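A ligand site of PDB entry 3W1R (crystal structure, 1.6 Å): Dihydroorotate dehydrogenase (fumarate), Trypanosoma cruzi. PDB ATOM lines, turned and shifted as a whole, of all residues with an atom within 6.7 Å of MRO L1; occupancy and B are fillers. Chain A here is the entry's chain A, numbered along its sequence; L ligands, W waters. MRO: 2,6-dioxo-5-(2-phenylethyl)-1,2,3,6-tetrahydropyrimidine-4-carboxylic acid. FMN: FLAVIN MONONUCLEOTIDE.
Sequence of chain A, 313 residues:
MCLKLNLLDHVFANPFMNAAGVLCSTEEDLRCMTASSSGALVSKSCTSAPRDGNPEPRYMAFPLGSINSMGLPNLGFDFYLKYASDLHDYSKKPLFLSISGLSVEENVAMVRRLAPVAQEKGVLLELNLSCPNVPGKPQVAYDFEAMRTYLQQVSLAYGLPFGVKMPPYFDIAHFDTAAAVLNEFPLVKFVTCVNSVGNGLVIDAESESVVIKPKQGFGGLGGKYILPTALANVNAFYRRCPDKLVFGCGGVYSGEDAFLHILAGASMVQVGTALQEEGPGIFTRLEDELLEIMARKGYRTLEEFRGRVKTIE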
ATOM      1  N   ALA A  20     -21.696  23.357   4.340  1.00  0.00           N
ATOM      2  CA  ALA A  20     -21.651  22.872   2.953  1.00  0.00           C
ATOM      3  C   ALA A  20     -22.515  23.695   2.021  1.00  0.00           C
ATOM      4  O   ALA A  20     -23.636  24.068   2.377  1.00  0.00           O
ATOM      5  CB  ALA A  20     -22.080  21.387   2.943  1.00  0.00           C
ATOM      6  N   LYS A  44     -18.384  21.560  -1.299  1.00  0.00           N
ATOM      7  CA  LYS A  44     -19.739  21.487  -1.758  1.00  0.00           C
ATOM      8  C   LYS A  44     -20.220  20.044  -1.933  1.00  0.00           C
ATOM      9  O   LYS A  44     -19.529  19.283  -2.618  1.00  0.00           O
ATOM     10  CB  LYS A  44     -19.777  22.251  -3.124  1.00  0.00           C
ATOM     11  CG  LYS A  44     -21.155  22.110  -3.849  1.00  0.00           C
ATOM     12  CD  LYS A  44     -22.365  22.805  -3.148  1.00  0.00           C
ATOM     13  CE  LYS A  44     -23.734  22.413  -3.839  1.00  0.00           C
ATOM     14  NZ  LYS A  44     -25.023  23.002  -3.181  1.00  0.00           N
ATOM     15  N   SER A  45     -21.440  19.784  -1.462  1.00  0.00           N
ATOM     16  CA  SER A  45     -22.043  18.409  -1.634  1.00  0.00           C
ATOM     17  C   SER A  45     -21.978  18.081  -3.112  1.00  0.00           C
ATOM     18  O   SER A  45     -22.377  18.885  -3.956  1.00  0.00           O
ATOM     19  CB  SER A  45     -23.500  18.373  -1.246  1.00  0.00           C
ATOM     20  OG  SER A  45     -23.499  18.516   0.205  1.00  0.00           O
ATOM     21  N   ARG A  51     -22.949  18.951 -12.070  1.00  0.00           N
ATOM     22  CA  ARG A  51     -24.276  19.461 -12.321  1.00  0.00           C
ATOM     23  C   ARG A  51     -24.276  20.951 -12.451  1.00  0.00           C
ATOM     24  O   ARG A  51     -23.603  21.673 -11.691  1.00  0.00           O
ATOM     25  CB  ARG A  51     -25.196  19.142 -11.110  1.00  0.00           C
ATOM     26  CG  ARG A  51     -25.499  17.626 -10.897  1.00  0.00           C
ATOM     27  CD  ARG A  51     -26.290  17.434  -9.603  1.00  0.00           C
ATOM     28  NE  ARG A  51     -27.532  18.213  -9.514  1.00  0.00           N
ATOM     29  CZ  ARG A  51     -28.713  17.754  -9.941  1.00  0.00           C
ATOM     30  NH1 ARG A  51     -28.797  16.574 -10.622  1.00  0.00           N
ATOM     31  NH2 ARG A  51     -29.809  18.468  -9.793  1.00  0.00           N
ATOM     32  N   ASN A  54     -30.079  24.387 -10.727  1.00  0.00           N
ATOM     33  CA  ASN A  54     -31.329  24.997 -11.233  1.00  0.00           C
ATOM     34  C   ASN A  54     -31.162  26.375 -11.850  1.00  0.00           C
ATOM     35  O   ASN A  54     -30.155  27.026 -11.699  1.00  0.00           O
ATOM     36  CB  ASN A  54     -32.240  25.140 -10.018  1.00  0.00           C
ATOM     37  CG  ASN A  54     -32.833  23.836  -9.578  1.00  0.00           C
ATOM     38  OD1 ASN A  54     -32.934  22.866 -10.350  1.00  0.00           O
ATOM     39  ND2 ASN A  54     -33.205  23.736  -8.271  1.00  0.00           N
ATOM     40  N   ASN A  68     -33.039  29.207  -0.627  1.00  0.00           N
ATOM     41  CA  ASN A  68     -32.279  28.708  -1.838  1.00  0.00           C
ATOM     42  C   ASN A  68     -32.981  27.445  -2.326  1.00  0.00           C
ATOM     43  O   ASN A  68     -33.419  26.548  -1.611  1.00  0.00           O
ATOM     44  CB  ASN A  68     -30.797  28.447  -1.521  1.00  0.00           C
ATOM     45  CG  ASN A  68     -30.588  27.087  -0.940  1.00  0.00           C
ATOM     46  OD1 ASN A  68     -30.466  26.077  -1.688  1.00  0.00           O
ATOM     47  ND2 ASN A  68     -30.439  27.003   0.392  1.00  0.00           N
ATOM     48  N   SER A  69     -32.974  27.290  -3.647  1.00  0.00           N
ATOM     49  CA  SER A  69     -33.202  26.031  -4.350  1.00  0.00           C
ATOM     50  C   SER A  69     -32.149  25.872  -5.473  1.00  0.00           C
ATOM     51  O   SER A  69     -32.443  25.977  -6.579  1.00  0.00           O
ATOM     52  CB  SER A  69     -34.635  25.910  -4.891  1.00  0.00           C
ATOM     53  OG  SER A  69     -35.552  25.826  -3.838  1.00  0.00           O
ATOM     54  N   MET A  70     -30.918  25.680  -5.029  1.00  0.00           N
ATOM     55  CA  MET A  70     -29.786  25.628  -5.906  1.00  0.00           C
ATOM     56  C   MET A  70     -29.808  24.507  -6.944  1.00  0.00           C
ATOM     57  O   MET A  70     -29.400  24.680  -8.045  1.00  0.00           O
ATOM     58  CB  MET A  70     -28.485  25.532  -5.136  1.00  0.00           C
ATOM     59  CG  MET A  70     -28.228  26.547  -4.083  1.00  0.00           C
ATOM     60  SD  MET A  70     -28.199  28.253  -4.702  1.00  0.00           S
ATOM     61  CE  MET A  70     -26.613  28.303  -5.564  1.00  0.00           C
ATOM     62  N   GLY A  71     -30.301  23.357  -6.537  1.00  0.00           N
ATOM     63  CA  GLY A  71     -30.290  22.195  -7.384  1.00  0.00           C
ATOM     64  C   GLY A  71     -29.009  21.390  -7.450  1.00  0.00           C
ATOM     65  O   GLY A  71     -28.709  20.776  -8.372  1.00  0.00           O
ATOM     66  N   LEU A  72     -28.280  21.497  -6.383  1.00  0.00           N
ATOM     67  CA  LEU A  72     -27.058  20.814  -6.241  1.00  0.00           C
ATOM     68  C   LEU A  72     -26.053  21.060  -7.351  1.00  0.00           C
ATOM     69  O   LEU A  72     -25.482  20.170  -7.851  1.00  0.00           O
ATOM     70  CB  LEU A  72     -27.338  19.310  -6.083  1.00  0.00           C
ATOM     71  CG  LEU A  72     -26.342  18.371  -5.407  1.00  0.00           C
ATOM     72  CD1 LEU A  72     -25.823  18.941  -4.115  1.00  0.00           C
ATOM     73  CD2 LEU A  72     -27.160  17.125  -5.033  1.00  0.00           C
ATOM     74  N   PRO A  73     -25.840  22.296  -7.694  1.00  0.00           N
ATOM     75  CA  PRO A  73     -24.779  22.537  -8.678  1.00  0.00           C
ATOM     76  C   PRO A  73     -23.386  22.164  -8.079  1.00  0.00           C
ATOM     77  O   PRO A  73     -23.149  22.503  -6.992  1.00  0.00           O
ATOM     78  CB  PRO A  73     -24.825  24.025  -8.909  1.00  0.00           C
ATOM     79  CG  PRO A  73     -25.280  24.577  -7.620  1.00  0.00           C
ATOM     80  CD  PRO A  73     -26.303  23.672  -7.132  1.00  0.00           C
ATOM     81  N   SER A 100     -23.546  13.960  -1.814  1.00  0.00           N
ATOM     82  CA  SER A 100     -24.997  13.982  -1.814  1.00  0.00           C
ATOM     83  C   SER A 100     -25.508  13.296  -3.056  1.00  0.00           C
ATOM     84  O   SER A 100     -26.203  13.885  -3.908  1.00  0.00           O
ATOM     85  CB  SER A 100     -25.446  15.454  -1.689  1.00  0.00           C
ATOM     86  OG  SER A 100     -26.865  15.548  -1.673  1.00  0.00           O
ATOM     87  N   LEU A 102     -27.727  10.988  -5.592  1.00  0.00           N
ATOM     88  CA  LEU A 102     -29.177  11.055  -5.812  1.00  0.00           C
ATOM     89  C   LEU A 102     -29.832   9.664  -5.578  1.00  0.00           C
ATOM     90  O   LEU A 102     -31.066   9.505  -5.723  1.00  0.00           O
ATOM     91  CB  LEU A 102     -29.490  11.612  -7.210  1.00  0.00           C
ATOM     92  CG  LEU A 102     -28.909  13.050  -7.404  1.00  0.00           C
ATOM     93  CD1 LEU A 102     -29.387  13.489  -8.803  1.00  0.00           C
ATOM     94  CD2 LEU A 102     -29.366  13.990  -6.362  1.00  0.00           C
ATOM     95  N   ASN A 128     -24.595  13.892   3.119  1.00  0.00           N
ATOM     96  CA  ASN A 128     -25.793  14.687   3.225  1.00  0.00           C
ATOM     97  C   ASN A 128     -27.015  13.838   3.072  1.00  0.00           C
ATOM     98  O   ASN A 128     -27.339  13.347   1.980  1.00  0.00           O
ATOM     99  CB  ASN A 128     -25.737  15.737   2.085  1.00  0.00           C
ATOM    100  CG  ASN A 128     -26.904  16.712   2.125  1.00  0.00           C
ATOM    101  OD1 ASN A 128     -27.693  16.764   3.007  1.00  0.00           O
ATOM    102  ND2 ASN A 128     -26.853  17.621   1.147  1.00  0.00           N
ATOM    103  N   SER A 130     -30.099  15.123   3.748  1.00  0.00           N
ATOM    104  CA  SER A 130     -31.253  16.019   3.662  1.00  0.00           C
ATOM    105  C   SER A 130     -31.220  16.350   2.288  1.00  0.00           C
ATOM    106  O   SER A 130     -30.827  17.454   1.896  1.00  0.00           O
ATOM    107  CB  SER A 130     -31.113  17.220   4.501  1.00  0.00           C
ATOM    108  OG  SER A 130     -32.022  18.182   4.122  1.00  0.00           O
ATOM    109  N   CYS A 131     -31.595  15.386   1.474  1.00  0.00           N
ATOM    110  CA  CYS A 131     -31.343  15.343   0.107  1.00  0.00           C
ATOM    111  C   CYS A 131     -32.473  14.497  -0.586  1.00  0.00           C
ATOM    112  O   CYS A 131     -32.806  13.370  -0.100  1.00  0.00           O
ATOM    113  CB  CYS A 131     -30.127  14.311   0.060  1.00  0.00           C
ATOM    114  SG  CYS A 131     -29.495  14.217  -1.665  1.00  0.00           S
ATOM    115  N   PRO A 132     -33.015  14.922  -1.775  1.00  0.00           N
ATOM    116  CA  PRO A 132     -33.924  14.004  -2.574  1.00  0.00           C
ATOM    117  C   PRO A 132     -33.516  12.544  -2.829  1.00  0.00           C
ATOM    118  O   PRO A 132     -32.343  12.228  -3.112  1.00  0.00           O
ATOM    119  CB  PRO A 132     -34.030  14.717  -3.956  1.00  0.00           C
ATOM    120  CG  PRO A 132     -32.889  15.708  -4.006  1.00  0.00           C
ATOM    121  CD  PRO A 132     -32.640  16.135  -2.561  1.00  0.00           C
ATOM    122  N   LYS A 165     -25.116  14.853   7.609  1.00  0.00           N
ATOM    123  CA  LYS A 165     -25.735  16.215   7.690  1.00  0.00           C
ATOM    124  C   LYS A 165     -27.271  15.967   7.690  1.00  0.00           C
ATOM    125  O   LYS A 165     -27.802  15.283   6.813  1.00  0.00           O
ATOM    126  CB  LYS A 165     -25.326  17.007   6.419  1.00  0.00           C
ATOM    127  CG  LYS A 165     -26.035  18.387   6.289  1.00  0.00           C
ATOM    128  CD  LYS A 165     -25.482  19.408   7.265  1.00  0.00           C
ATOM    129  CE  LYS A 165     -25.934  20.815   6.929  1.00  0.00           C
ATOM    130  NZ  LYS A 165     -25.246  21.350   5.744  1.00  0.00           N
ATOM    131  N   ASN A 195     -29.335  21.094   8.305  1.00  0.00           N
ATOM    132  CA  ASN A 195     -29.525  21.660   6.950  1.00  0.00           C
ATOM    133  C   ASN A 195     -30.658  22.726   6.953  1.00  0.00           C
ATOM    134  O   ASN A 195     -31.290  22.981   7.984  1.00  0.00           O
ATOM    135  CB  ASN A 195     -29.869  20.456   5.986  1.00  0.00           C
ATOM    136  CG  ASN A 195     -29.361  20.702   4.563  1.00  0.00           C
ATOM    137  OD1 ASN A 195     -29.520  21.780   3.997  1.00  0.00           O
ATOM    138  ND2 ASN A 195     -28.622  19.691   4.031  1.00  0.00           N
ATOM    139  N   SER A 196     -30.960  23.308   5.782  1.00  0.00           N
ATOM    140  CA  SER A 196     -31.991  24.344   5.777  1.00  0.00           C
ATOM    141  C   SER A 196     -33.363  23.845   6.183  1.00  0.00           C
ATOM    142  O   SER A 196     -33.716  22.682   6.057  1.00  0.00           O
ATOM    143  CB  SER A 196     -32.053  24.996   4.365  1.00  0.00           C
ATOM    144  OG  SER A 196     -31.957  24.108   3.359  1.00  0.00           O
ATOM    145  N   LYS A 215     -39.017  25.706  -8.394  1.00  0.00           N
ATOM    146  CA  LYS A 215     -39.995  25.229  -7.413  1.00  0.00           C
ATOM    147  C   LYS A 215     -41.070  26.273  -7.040  1.00  0.00           C
ATOM    148  O   LYS A 215     -41.518  26.306  -5.965  1.00  0.00           O
ATOM    149  CB  LYS A 215     -39.314  24.715  -6.137  1.00  0.00           C
ATOM    150  CG  LYS A 215     -38.407  23.503  -6.386  1.00  0.00           C
ATOM    151  CD  LYS A 215     -37.677  23.051  -5.122  1.00  0.00           C
ATOM    152  CE  LYS A 215     -38.626  22.867  -3.979  1.00  0.00           C
ATOM    153  NZ  LYS A 215     -37.910  22.195  -2.911  1.00  0.00           N
ATOM    154  N   GLY A 220     -35.238  26.184   0.640  1.00  0.00           N
ATOM    155  CA  GLY A 220     -34.772  26.000   1.983  1.00  0.00           C
ATOM    156  C   GLY A 220     -34.363  27.312   2.667  1.00  0.00           C
ATOM    157  O   GLY A 220     -33.672  28.101   2.078  1.00  0.00           O
ATOM    158  N   LEU A 221     -34.721  27.435   3.937  1.00  0.00           N
ATOM    159  CA  LEU A 221     -34.401  28.603   4.701  1.00  0.00           C
ATOM    160  C   LEU A 221     -33.186  28.482   5.599  1.00  0.00           C
ATOM    161  O   LEU A 221     -33.000  27.511   6.233  1.00  0.00           O
ATOM    162  CB  LEU A 221     -35.599  28.962   5.570  1.00  0.00           C
ATOM    163  CG  LEU A 221     -36.941  29.093   4.861  1.00  0.00           C
ATOM    164  CD1 LEU A 221     -37.993  29.139   5.958  1.00  0.00           C
ATOM    165  CD2 LEU A 221     -36.980  30.319   3.994  1.00  0.00           C
HETATM  166  OAA MRO L   1     -28.211  22.511  -3.667  1.00  0.00           O
HETATM  167  CAN MRO L   1     -29.250  22.662  -2.996  1.00  0.00           C
HETATM  168  OAD MRO L   1     -30.357  23.144  -3.298  1.00  0.00           O
HETATM  169  CAQ MRO L   1     -29.152  22.372  -1.469  1.00  0.00           C
HETATM  170  NAL MRO L   1     -29.547  23.514  -0.693  1.00  0.00           N
HETATM  171  CAR MRO L   1     -29.617  23.395   0.688  1.00  0.00           C
HETATM  172  OAB MRO L   1     -29.967  24.340   1.417  1.00  0.00           O
HETATM  173  NAM MRO L   1     -29.201  22.204   1.265  1.00  0.00           N
HETATM  174  CAS MRO L   1     -28.812  21.061   0.508  1.00  0.00           C
HETATM  175  OAC MRO L   1     -28.494  20.019   1.068  1.00  0.00           O
HETATM  176  CAP MRO L   1     -28.820  21.188  -0.900  1.00  0.00           C
HETATM  177  CAK MRO L   1     -28.442  20.088  -1.712  1.00  0.00           C
HETATM  178  CAJ MRO L   1     -29.571  18.973  -1.632  1.00  0.00           C
HETATM  179  CAO MRO L   1     -30.731  19.347  -2.223  1.00  0.00           C
HETATM  180  CAH MRO L   1     -30.728  19.249  -3.638  1.00  0.00           C
HETATM  181  CAF MRO L   1     -31.989  19.596  -4.192  1.00  0.00           C
HETATM  182  CAE MRO L   1     -33.128  20.026  -3.489  1.00  0.00           C
HETATM  183  CAG MRO L   1     -33.180  20.157  -2.058  1.00  0.00           C
HETATM  184  CAI MRO L   1     -31.911  19.771  -1.471  1.00  0.00           C
HETATM  185  N1  FMN L   2     -26.152  21.886   2.798  1.00  0.00           N
HETATM  186  C2  FMN L   2     -25.593  20.714   2.365  1.00  0.00           C
HETATM  187  O2  FMN L   2     -25.378  19.830   3.205  1.00  0.00           O
HETATM  188  N3  FMN L   2     -25.072  20.569   1.119  1.00  0.00           N
HETATM  189  C4  FMN L   2     -25.150  21.564   0.185  1.00  0.00           C
HETATM  190  O4  FMN L   2     -24.677  21.435  -1.002  1.00  0.00           O
HETATM  191  C4A FMN L   2     -25.744  22.839   0.568  1.00  0.00           C
HETATM  192  N5  FMN L   2     -25.865  23.818  -0.318  1.00  0.00           N
HETATM  193  C5A FMN L   2     -26.253  25.042   0.124  1.00  0.00           C
HETATM  194  C6  FMN L   2     -26.174  26.158  -0.749  1.00  0.00           C
HETATM  195  C7  FMN L   2     -26.610  27.398  -0.312  1.00  0.00           C
HETATM  196  C7M FMN L   2     -26.568  28.590  -1.258  1.00  0.00           C
HETATM  197  C8  FMN L   2     -27.083  27.572   1.058  1.00  0.00           C
HETATM  198  C8M FMN L   2     -27.561  28.901   1.548  1.00  0.00           C
HETATM  199  C9  FMN L   2     -27.142  26.459   1.939  1.00  0.00           C
HETATM  200  C9A FMN L   2     -26.742  25.232   1.490  1.00  0.00           C
HETATM  201  N10 FMN L   2     -26.796  24.092   2.328  1.00  0.00           N
HETATM  202  C10 FMN L   2     -26.262  22.912   1.929  1.00  0.00           C
HETATM  203  C1' FMN L   2     -27.251  24.229   3.703  1.00  0.00           C
HETATM  204  C2' FMN L   2     -26.235  24.906   4.623  1.00  0.00           C
HETATM  205  O2' FMN L   2     -25.157  23.958   4.712  1.00  0.00           O
HETATM  206  C3' FMN L   2     -26.736  25.085   6.015  1.00  0.00           C
HETATM  207  O3' FMN L   2     -27.181  23.798   6.529  1.00  0.00           O
HETATM  208  C4' FMN L   2     -28.043  25.964   6.002  1.00  0.00           C
HETATM  209  O4' FMN L   2     -27.856  27.095   5.093  1.00  0.00           O
HETATM  210  C5' FMN L   2     -28.315  26.533   7.429  1.00  0.00           C
HETATM  211  O5' FMN L   2     -27.204  27.282   7.973  1.00  0.00           O
HETATM  212  P   FMN L   2     -27.259  28.914   7.990  1.00  0.00           P
HETATM  213  O1P FMN L   2     -25.894  29.332   8.522  1.00  0.00           O
HETATM  214  O2P FMN L   2     -28.455  29.290   8.808  1.00  0.00           O
HETATM  215  O3P FMN L   2     -27.447  29.331   6.501  1.00  0.00           O
HETATM  216  O   HOH W   1     -32.966  22.855  -5.067  1.00  0.00           O
HETATM  217  O   HOH W   2     -32.658  23.644  -1.441  1.00  0.00           O
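The side-chain amide oxygen (OD1) of Asn 195 is in hydrogen-bond range of a nitrogen (NAM) of MRO L1 (2.8 Å). OAB of MRO L1 lies within hydrogen-bond range of OG of Ser 196 (2.8 Å). The side-chain amide nitrogen (ND2) of Asn 68 is in hydrogen-bond range of an oxygen (OAB) of MRO L1. The backbone NH (N) of Leu 72 lies within hydrogen-bond range of an oxygen (OAA) of MRO L1 (2.9 Å). The side-chain amide nitrogen (ND2) of Asn 128 sits at hydrogen-bond distance from an oxygen (OAC) of MRO L1, at 2.9 Å. N of Met 70 is in hydrogen-bond range of OAD of MRO L1, 3.1 Å away. OAD of MRO L1 sits at hydrogen-bond distance from N of Gly 71. NZ of Lys 44 is in salt-bridge range of OAA of MRO L1. ND2 of Asn 195 is in hydrogen-bond range of O2 of FMN L2. An oxygen (O2) of FMN L2 lies within hydrogen-bond range of the side-chain amide nitrogen of Asn 128 (3.4 Å). NZ of Lys 44 sits at hydrogen-bond distance from O4 of FMN L2, 2.7 Å away. The side-chain hydroxyl (OG) of Ser 45 lies within hydrogen-bond range of a nitrogen (N3) of FMN L2, 2.7 Å away. An oxygen (O2') of FMN L2 lies within hydrogen-bond range of the side-chain amino group of Lys 165. The backbone carbonyl oxygen (O) of Ala 20 is in hydrogen-bond range of an oxygen (O2') of FMN L2 (2.8 Å).
A nitrogen (NAM) of MRO L1 sits close to a nitrogen (N1) of FMN L2, 3.4 Å away.
The side-chain amide nitrogen of Asn 195 sits at hydrogen-bond distance from the side-chain amide oxygen of Asn 128 (3.2 Å). The backbone NH of Met 70 sits close to the side-chain amide oxygen of Asn 68 (3.4 Å). The backbone carbonyl oxygen of Asn 68 lies within hydrogen-bond range of the backbone NH of Gly 220. The backbone carbonyl oxygen (O) of Leu 72 lies within hydrogen-bond range of the guanidinium group (NE) of Arg 51, 3.3 Å away. The backbone carbonyl oxygen of Met 70 lies within hydrogen-bond range of the backbone NH of Asn 54, 2.8 Å away. The backbone NH (N) of Gly 71 lies close to the side-chain amide nitrogen (ND2) of Asn 54 (3.4 Å). The backbone carbonyl oxygen (O) of Gly 71 is in hydrogen-bond range of the guanidinium group (NH2) of Arg 51, at 2.9 Å. ND2 of Asn 54 sits at hydrogen-bond distance from O of Ser 69, at 2.9 Å.
Ser 69 touches MRO L1 (C to OAD, 3.9 Å). O of Ser 130 touches OAC of MRO L1, 3.6 Å away. Pro 132 touches MRO L1 (CD to CAO, 3.8 Å). Of the 23 residues printed, 11 come within 4 Å of MRO L1. The nearest printed residue that does not touch MRO L1 is Pro 73 (4.1 Å).
Water W2 lies within hydrogen-bond range of an oxygen (OAD) of MRO L1 and the backbone carbonyl oxygen of Asn 68.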
